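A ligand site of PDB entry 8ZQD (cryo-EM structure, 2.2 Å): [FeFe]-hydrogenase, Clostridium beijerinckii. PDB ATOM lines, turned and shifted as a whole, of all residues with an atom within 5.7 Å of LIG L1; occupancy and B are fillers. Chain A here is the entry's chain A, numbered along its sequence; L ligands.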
ATOM      1  N   ALA A 292     -24.813  23.330 -26.350  1.00  0.00           N
ATOM      2  CA  ALA A 292     -24.471  24.178 -25.225  1.00  0.00           C
ATOM      3  C   ALA A 292     -25.272  23.769 -23.991  1.00  0.00           C
ATOM      4  O   ALA A 292     -26.369  23.212 -24.112  1.00  0.00           O
ATOM      5  CB  ALA A 292     -24.721  25.640 -25.568  1.00  0.00           C
ATOM      6  N   PRO A 293     -24.739  24.024 -22.792  1.00  0.00           N
ATOM      7  CA  PRO A 293     -25.490  23.672 -21.568  1.00  0.00           C
ATOM      8  C   PRO A 293     -26.866  24.317 -21.477  1.00  0.00           C
ATOM      9  O   PRO A 293     -27.813  23.676 -21.016  1.00  0.00           O
ATOM     10  CB  PRO A 293     -24.560  24.154 -20.456  1.00  0.00           C
ATOM     11  CG  PRO A 293     -23.201  24.148 -21.051  1.00  0.00           C
ATOM     12  CD  PRO A 293     -23.360  24.457 -22.504  1.00  0.00           C
ATOM     13  N   ALA A 294     -27.000  25.563 -21.908  1.00  0.00           N
ATOM     14  CA  ALA A 294     -28.261  26.293 -21.727  1.00  0.00           C
ATOM     15  C   ALA A 294     -29.339  25.837 -22.696  1.00  0.00           C
ATOM     16  O   ALA A 294     -30.517  26.123 -22.460  1.00  0.00           O
ATOM     17  CB  ALA A 294     -28.023  27.795 -21.888  1.00  0.00           C
ATOM     18  N   VAL A 295     -28.985  25.140 -23.776  1.00  0.00           N
ATOM     19  CA  VAL A 295     -29.976  24.705 -24.754  1.00  0.00           C
ATOM     20  C   VAL A 295     -30.927  23.680 -24.136  1.00  0.00           C
ATOM     21  O   VAL A 295     -32.143  23.728 -24.333  1.00  0.00           O
ATOM     22  CB  VAL A 295     -29.290  24.157 -26.009  1.00  0.00           C
ATOM     23  CG1 VAL A 295     -30.304  23.514 -26.940  1.00  0.00           C
ATOM     24  CG2 VAL A 295     -28.529  25.260 -26.729  1.00  0.00           C
ATOM     25  N   THR A 330     -21.232  20.436 -25.550  1.00  0.00           N
ATOM     26  CA  THR A 330     -20.269  21.497 -25.318  1.00  0.00           C
ATOM     27  C   THR A 330     -19.782  21.510 -23.873  1.00  0.00           C
ATOM     28  O   THR A 330     -18.767  22.149 -23.570  1.00  0.00           O
ATOM     29  CB  THR A 330     -20.868  22.850 -25.700  1.00  0.00           C
ATOM     30  OG1 THR A 330     -21.488  22.755 -26.984  1.00  0.00           O
ATOM     31  CG2 THR A 330     -19.799  23.942 -25.756  1.00  0.00           C
ATOM     32  N   SER A 331     -20.470  20.820 -22.971  1.00  0.00           N
ATOM     33  CA  SER A 331     -20.008  20.754 -21.591  1.00  0.00           C
ATOM     34  C   SER A 331     -18.692  19.986 -21.465  1.00  0.00           C
ATOM     35  O   SER A 331     -17.925  20.216 -20.534  1.00  0.00           O
ATOM     36  CB  SER A 331     -21.087  20.137 -20.711  1.00  0.00           C
ATOM     37  OG  SER A 331     -22.185  21.020 -20.555  1.00  0.00           O
ATOM     38  N   GLY A 333     -16.246  20.330 -23.741  1.00  0.00           N
ATOM     39  CA  GLY A 333     -15.331  21.416 -23.981  1.00  0.00           C
ATOM     40  C   GLY A 333     -15.254  22.380 -22.815  1.00  0.00           C
ATOM     41  O   GLY A 333     -14.215  23.004 -22.581  1.00  0.00           O
ATOM     42  N   ALA A 334     -16.350  22.527 -22.065  1.00  0.00           N
ATOM     43  CA  ALA A 334     -16.324  23.340 -20.860  1.00  0.00           C
ATOM     44  C   ALA A 334     -15.409  22.746 -19.800  1.00  0.00           C
ATOM     45  O   ALA A 334     -14.671  23.479 -19.133  1.00  0.00           O
ATOM     46  CB  ALA A 334     -17.746  23.508 -20.305  1.00  0.00           C
ATOM     47  N   CYS A 367     -14.843  33.043 -22.424  1.00  0.00           N
ATOM     48  CA  CYS A 367     -15.803  32.137 -23.052  1.00  0.00           C
ATOM     49  C   CYS A 367     -16.936  32.862 -23.765  1.00  0.00           C
ATOM     50  O   CYS A 367     -17.533  32.304 -24.681  1.00  0.00           O
ATOM     51  CB  CYS A 367     -16.368  31.191 -21.996  1.00  0.00           C
ATOM     52  SG  CYS A 367     -16.834  31.997 -20.454  1.00  0.00           S
ATOM     53  N   CYS A 368     -17.239  34.099 -23.369  1.00  0.00           N
ATOM     54  CA  CYS A 368     -18.327  34.848 -23.996  1.00  0.00           C
ATOM     55  C   CYS A 368     -17.811  35.628 -25.190  1.00  0.00           C
ATOM     56  O   CYS A 368     -17.014  36.555 -25.031  1.00  0.00           O
ATOM     57  CB  CYS A 368     -18.978  35.780 -22.983  1.00  0.00           C
ATOM     58  SG  CYS A 368     -20.346  36.766 -23.646  1.00  0.00           S
ATOM     59  N   PRO A 369     -18.232  35.278 -26.416  1.00  0.00           N
ATOM     60  CA  PRO A 369     -17.737  36.001 -27.597  1.00  0.00           C
ATOM     61  C   PRO A 369     -18.246  37.424 -27.695  1.00  0.00           C
ATOM     62  O   PRO A 369     -17.538  38.285 -28.229  1.00  0.00           O
ATOM     63  CB  PRO A 369     -18.246  35.151 -28.760  1.00  0.00           C
ATOM     64  CG  PRO A 369     -19.472  34.492 -28.231  1.00  0.00           C
ATOM     65  CD  PRO A 369     -19.215  34.243 -26.771  1.00  0.00           C
ATOM     66  N   SER A 391     -12.995  29.536 -25.951  1.00  0.00           N
ATOM     67  CA  SER A 391     -14.284  29.187 -25.385  1.00  0.00           C
ATOM     68  C   SER A 391     -14.503  27.685 -25.492  1.00  0.00           C
ATOM     69  O   SER A 391     -13.829  27.016 -26.282  1.00  0.00           O
ATOM     70  CB  SER A 391     -15.403  29.946 -26.103  1.00  0.00           C
ATOM     71  OG  SER A 391     -15.671  29.369 -27.368  1.00  0.00           O
ATOM     72  N   PRO A 392     -15.390  27.124 -24.674  1.00  0.00           N
ATOM     73  CA  PRO A 392     -15.654  25.677 -24.773  1.00  0.00           C
ATOM     74  C   PRO A 392     -16.065  25.224 -26.169  1.00  0.00           C
ATOM     75  O   PRO A 392     -15.647  24.145 -26.602  1.00  0.00           O
ATOM     76  CB  PRO A 392     -16.790  25.469 -23.755  1.00  0.00           C
ATOM     77  CG  PRO A 392     -16.553  26.523 -22.740  1.00  0.00           C
ATOM     78  CD  PRO A 392     -16.046  27.719 -23.497  1.00  0.00           C
ATOM     79  N   MET A 393     -16.857  26.030 -26.888  1.00  0.00           N
ATOM     80  CA  MET A 393     -17.270  25.649 -28.228  1.00  0.00           C
ATOM     81  C   MET A 393     -16.072  25.499 -29.154  1.00  0.00           C
ATOM     82  O   MET A 393     -15.942  24.494 -29.866  1.00  0.00           O
ATOM     83  CB  MET A 393     -18.267  26.670 -28.782  1.00  0.00           C
ATOM     84  CG  MET A 393     -18.589  26.494 -30.262  1.00  0.00           C
ATOM     85  SD  MET A 393     -19.542  27.857 -30.950  1.00  0.00           S
ATOM     86  CE  MET A 393     -18.235  28.991 -31.423  1.00  0.00           C
ATOM     87  N   GLU A 394     -15.165  26.476 -29.139  1.00  0.00           N
ATOM     88  CA  GLU A 394     -13.997  26.413 -30.016  1.00  0.00           C
ATOM     89  C   GLU A 394     -12.993  25.352 -29.566  1.00  0.00           C
ATOM     90  O   GLU A 394     -12.363  24.717 -30.417  1.00  0.00           O
ATOM     91  CB  GLU A 394     -13.329  27.781 -30.111  1.00  0.00           C
ATOM     92  CG  GLU A 394     -14.091  28.763 -30.993  1.00  0.00           C
ATOM     93  CD  GLU A 394     -14.146  28.344 -32.446  1.00  0.00           C
ATOM     94  OE1 GLU A 394     -13.330  27.497 -32.866  1.00  0.00           O
ATOM     95  OE2 GLU A 394     -15.015  28.852 -33.176  1.00  0.00           O
ATOM     96  N   MET A 421     -26.279  26.537 -30.179  1.00  0.00           N
ATOM     97  CA  MET A 421     -25.970  27.511 -29.154  1.00  0.00           C
ATOM     98  C   MET A 421     -27.185  28.373 -28.858  1.00  0.00           C
ATOM     99  O   MET A 421     -28.051  28.562 -29.715  1.00  0.00           O
ATOM    100  CB  MET A 421     -24.803  28.414 -29.602  1.00  0.00           C
ATOM    101  CG  MET A 421     -23.537  27.652 -29.927  1.00  0.00           C
ATOM    102  SD  MET A 421     -22.609  27.206 -28.443  1.00  0.00           S
ATOM    103  CE  MET A 421     -22.448  25.438 -28.676  1.00  0.00           C
ATOM    104  N   PRO A 422     -27.281  28.899 -27.638  1.00  0.00           N
ATOM    105  CA  PRO A 422     -28.325  29.875 -27.307  1.00  0.00           C
ATOM    106  C   PRO A 422     -27.945  31.314 -27.616  1.00  0.00           C
ATOM    107  O   PRO A 422     -28.627  32.225 -27.143  1.00  0.00           O
ATOM    108  CB  PRO A 422     -28.475  29.679 -25.802  1.00  0.00           C
ATOM    109  CG  PRO A 422     -27.092  29.381 -25.346  1.00  0.00           C
ATOM    110  CD  PRO A 422     -26.452  28.580 -26.462  1.00  0.00           C
ATOM    111  N   CYS A 423     -26.890  31.534 -28.391  1.00  0.00           N
ATOM    112  CA  CYS A 423     -26.234  32.836 -28.489  1.00  0.00           C
ATOM    113  C   CYS A 423     -26.157  33.301 -29.929  1.00  0.00           C
ATOM    114  O   CYS A 423     -25.872  32.502 -30.830  1.00  0.00           O
ATOM    115  CB  CYS A 423     -24.827  32.763 -27.874  1.00  0.00           C
ATOM    116  SG  CYS A 423     -23.792  34.172 -28.229  1.00  0.00           S
ATOM    117  N   LYS A 426     -22.237  33.617 -30.936  1.00  0.00           N
ATOM    118  CA  LYS A 426     -21.509  32.384 -31.256  1.00  0.00           C
ATOM    119  C   LYS A 426     -21.310  32.235 -32.744  1.00  0.00           C
ATOM    120  O   LYS A 426     -20.306  31.656 -33.178  1.00  0.00           O
ATOM    121  CB  LYS A 426     -22.249  31.176 -30.687  1.00  0.00           C
ATOM    122  CG  LYS A 426     -22.084  31.001 -29.188  1.00  0.00           C
ATOM    123  CD  LYS A 426     -20.658  30.610 -28.832  1.00  0.00           C
ATOM    124  CE  LYS A 426     -20.358  30.889 -27.366  1.00  0.00           C
ATOM    125  NZ  LYS A 426     -18.905  30.818 -27.061  1.00  0.00           N
ATOM    126  N   GLU A 429     -18.251  34.266 -33.389  1.00  0.00           N
ATOM    127  CA  GLU A 429     -17.078  33.567 -32.879  1.00  0.00           C
ATOM    128  C   GLU A 429     -16.674  32.435 -33.813  1.00  0.00           C
ATOM    129  O   GLU A 429     -15.490  32.256 -34.122  1.00  0.00           O
ATOM    130  CB  GLU A 429     -17.341  33.028 -31.477  1.00  0.00           C
ATOM    131  CG  GLU A 429     -16.061  32.563 -30.791  1.00  0.00           C
ATOM    132  CD  GLU A 429     -16.316  31.932 -29.435  1.00  0.00           C
ATOM    133  OE1 GLU A 429     -17.480  31.949 -28.973  1.00  0.00           O
ATOM    134  OE2 GLU A 429     -15.352  31.424 -28.839  1.00  0.00           O
ATOM    135  N   GLY A 482     -18.969  21.320 -15.545  1.00  0.00           N
ATOM    136  CA  GLY A 482     -19.104  21.733 -16.929  1.00  0.00           C
ATOM    137  C   GLY A 482     -20.519  22.117 -17.320  1.00  0.00           C
ATOM    138  O   GLY A 482     -20.692  22.903 -18.252  1.00  0.00           O
ATOM    139  N   PHE A 485     -21.981  25.941 -16.689  1.00  0.00           N
ATOM    140  CA  PHE A 485     -21.492  27.046 -17.512  1.00  0.00           C
ATOM    141  C   PHE A 485     -22.639  27.903 -18.029  1.00  0.00           C
ATOM    142  O   PHE A 485     -22.522  29.140 -18.079  1.00  0.00           O
ATOM    143  CB  PHE A 485     -20.687  26.485 -18.689  1.00  0.00           C
ATOM    144  CG  PHE A 485     -19.208  26.543 -18.494  1.00  0.00           C
ATOM    145  CD1 PHE A 485     -18.619  26.016 -17.349  1.00  0.00           C
ATOM    146  CD2 PHE A 485     -18.381  27.106 -19.460  1.00  0.00           C
ATOM    147  CE1 PHE A 485     -17.253  26.071 -17.168  1.00  0.00           C
ATOM    148  CE2 PHE A 485     -17.021  27.165 -19.285  1.00  0.00           C
ATOM    149  CZ  PHE A 485     -16.446  26.638 -18.142  1.00  0.00           C
ATOM    150  N   GLY A 486     -23.762  27.282 -18.384  1.00  0.00           N
ATOM    151  CA  GLY A 486     -24.857  27.971 -19.050  1.00  0.00           C
ATOM    152  C   GLY A 486     -25.515  29.075 -18.245  1.00  0.00           C
ATOM    153  O   GLY A 486     -26.247  29.887 -18.827  1.00  0.00           O
ATOM    154  N   VAL A 491     -19.076  29.403 -14.767  1.00  0.00           N
ATOM    155  CA  VAL A 491     -17.707  29.257 -15.249  1.00  0.00           C
ATOM    156  C   VAL A 491     -16.714  29.476 -14.121  1.00  0.00           C
ATOM    157  O   VAL A 491     -15.802  28.660 -13.898  1.00  0.00           O
ATOM    158  CB  VAL A 491     -17.449  30.232 -16.416  1.00  0.00           C
ATOM    159  CG1 VAL A 491     -16.046  30.026 -16.978  1.00  0.00           C
ATOM    160  CG2 VAL A 491     -18.490  30.063 -17.503  1.00  0.00           C
ATOM    161  N   MET A 565     -20.287  37.761 -18.335  1.00  0.00           N
ATOM    162  CA  MET A 565     -21.313  37.336 -19.270  1.00  0.00           C
ATOM    163  C   MET A 565     -21.908  38.565 -19.948  1.00  0.00           C
ATOM    164  O   MET A 565     -21.900  39.672 -19.389  1.00  0.00           O
ATOM    165  CB  MET A 565     -22.424  36.557 -18.559  1.00  0.00           C
ATOM    166  CG  MET A 565     -21.975  35.218 -18.007  1.00  0.00           C
ATOM    167  SD  MET A 565     -20.897  34.325 -19.132  1.00  0.00           S
ATOM    168  CE  MET A 565     -22.044  33.144 -19.800  1.00  0.00           C
ATOM    169  N   CYS A 571     -25.906  32.271 -20.255  1.00  0.00           N
ATOM    170  CA  CYS A 571     -26.313  31.767 -21.563  1.00  0.00           C
ATOM    171  C   CYS A 571     -27.767  31.316 -21.587  1.00  0.00           C
ATOM    172  O   CYS A 571     -28.347  31.194 -22.670  1.00  0.00           O
ATOM    173  CB  CYS A 571     -25.401  30.621 -21.996  1.00  0.00           C
ATOM    174  SG  CYS A 571     -23.675  31.095 -22.211  1.00  0.00           S
ATOM    175  N   ILE A 572     -28.371  31.051 -20.422  1.00  0.00           N
ATOM    176  CA  ILE A 572     -29.783  30.699 -20.400  1.00  0.00           C
ATOM    177  C   ILE A 572     -30.648  31.872 -20.848  1.00  0.00           C
ATOM    178  O   ILE A 572     -31.774  31.664 -21.317  1.00  0.00           O
ATOM    179  CB  ILE A 572     -30.192  30.210 -18.986  1.00  0.00           C
ATOM    180  CG1 ILE A 572     -29.640  31.116 -17.893  1.00  0.00           C
ATOM    181  CG2 ILE A 572     -29.740  28.772 -18.774  1.00  0.00           C
ATOM    182  CD1 ILE A 572     -30.537  32.283 -17.525  1.00  0.00           C
HETATM  183 FE1  LIG L   1     -22.621  29.402 -23.321  1.00  0.00          FE
HETATM  184 FE2  LIG L   1     -20.419  28.161 -23.343  1.00  0.00          FE
HETATM  185  S1  LIG L   1     -21.615  28.634 -21.423  1.00  0.00           S
HETATM  186  S2  LIG L   1     -20.619  30.390 -23.855  1.00  0.00           S
HETATM  187  O1  LIG L   1     -23.575  30.263 -25.994  1.00  0.00           O
HETATM  188  N1  LIG L   1     -24.789  27.415 -22.574  1.00  0.00           N
HETATM  189  O2  LIG L   1     -21.807  27.023 -25.331  1.00  0.00           O
HETATM  190  N2  LIG L   1     -18.468  28.215 -25.704  1.00  0.00           N
HETATM  191  O3  LIG L   1     -19.925  25.412 -22.402  1.00  0.00           O
HETATM  192  C1  LIG L   1     -23.104  29.816 -24.942  1.00  0.00           C
HETATM  193  C2  LIG L   1     -23.922  28.207 -22.885  1.00  0.00           C
HETATM  194  C3  LIG L   1     -21.666  27.419 -24.216  1.00  0.00           C
HETATM  195  C4  LIG L   1     -19.169  28.102 -24.814  1.00  0.00           C
HETATM  196  C5  LIG L   1     -20.149  26.531 -22.720  1.00  0.00           C
HETATM  197  C6  LIG L   1     -20.031  31.435 -22.400  1.00  0.00           C
HETATM  198  N3  LIG L   1     -19.631  30.677 -21.178  1.00  0.00           N
HETATM  199  C7  LIG L   1     -20.734  29.971 -20.487  1.00  0.00           C
HETATM  200 FE1  LG2 L   2     -22.231  35.546 -23.935  1.00  0.00          FE
HETATM  201 FE2  LG2 L   2     -23.698  33.093 -23.281  1.00  0.00          FE
HETATM  202 FE3  LG2 L   2     -23.682  34.054 -25.974  1.00  0.00          FE
HETATM  203 FE4  LG2 L   2     -25.106  35.697 -23.901  1.00  0.00          FE
HETATM  204  S1  LG2 L   2     -25.310  33.738 -24.596  1.00  0.00           S
HETATM  205  S2  LG2 L   2     -23.649  36.120 -25.410  1.00  0.00           S
HETATM  206  S3  LG2 L   2     -23.663  35.073 -22.441  1.00  0.00           S
HETATM  207  S4  LG2 L   2     -22.077  33.562 -24.635  1.00  0.00           S
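The side-chain sulfur (SG) of Cys 571 is bound to an iron atom (FE1) of LIG L1, at 2.3 Å. N of Ala 294 sits at hydrogen-bond distance from N1 of LIG L1, at 3.0 Å. A nitrogen (N2) of LIG L1 is in hydrogen-bond range of the backbone NH of Met 393 (3.0 Å). NZ of Lys 426 lies within hydrogen-bond range of N2 of LIG L1, at 3.0 Å. The side-chain sulfur (SG) of Cys 367 sits at hydrogen-bond distance from a nitrogen (N3) of LIG L1 (3.2 Å). A nitrogen (N2) of LIG L1 sits at hydrogen-bond distance from the side-chain hydroxyl of Ser 391 (3.5 Å). FE2 of LG2 L2 is bound by SG of Cys 571. FE3 of LG2 L2 is bound by SG of Cys 423 (2.3 Å). The side-chain sulfur (SG) of Cys 368 is bound to an iron atom (FE1) of LG2 L2, at 2.3 Å.
The backbone NH (N) of Cys 571 is in hydrogen-bond range of the backbone carbonyl oxygen (O) of Gly 486 (2.8 Å). The side-chain amino group (NZ) of Lys 426 sits at hydrogen-bond distance from the backbone carbonyl oxygen (O) of Cys 367 (3.1 Å). The backbone NH (N) of Lys 426 lies close to the side-chain sulfur (SG) of Cys 423 (3.2 Å). The side-chain amino group of Lys 426 lies within salt-bridge range of the side-chain carboxylate of Glu 429 (2.6 Å). N of Ala 292 lies within hydrogen-bond range of OG1 of Thr 330 (3.4 Å). OG of Ser 391 sits at hydrogen-bond distance from OE2 of Glu 429 (2.5 Å). The side-chain hydroxyl (OG) of Ser 391 sits at hydrogen-bond distance from the backbone NH (N) of Glu 394 (3.4 Å). The backbone carbonyl oxygen (O) of Gly 486 lies within hydrogen-bond range of the backbone NH (N) of Ile 572 (2.9 Å).
N of Pro 293 lies close to N1 of LIG L1. The backbone nitrogen of Pro 392 sits close to a nitrogen (N2) of LIG L1 (3.4 Å). The side-chain sulfur (SD) of Met 421 lies close to an oxygen (O2) of LIG L1 (3.2 Å). The backbone carbonyl oxygen of Phe 485 lies close to a sulfur (S1) of LIG L1, 3.5 Å away. Merely in contact with LIG L1: Ala 292, Thr 330, Ala 334, Cys 368, Pro 422, Cys 423, Gly 486, Val 491 and Met 565. Hydrophobic or aromatic side chains that line LIG L1: Ala 292, Pro 293, Ala 294, Ala 334, Pro 392, Met 393, Met 421, Pro 422, Phe 485, Val 491 and Met 565. The nearest printed residue that does not touch LIG L1 is Ser 331 (4.7 Å).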
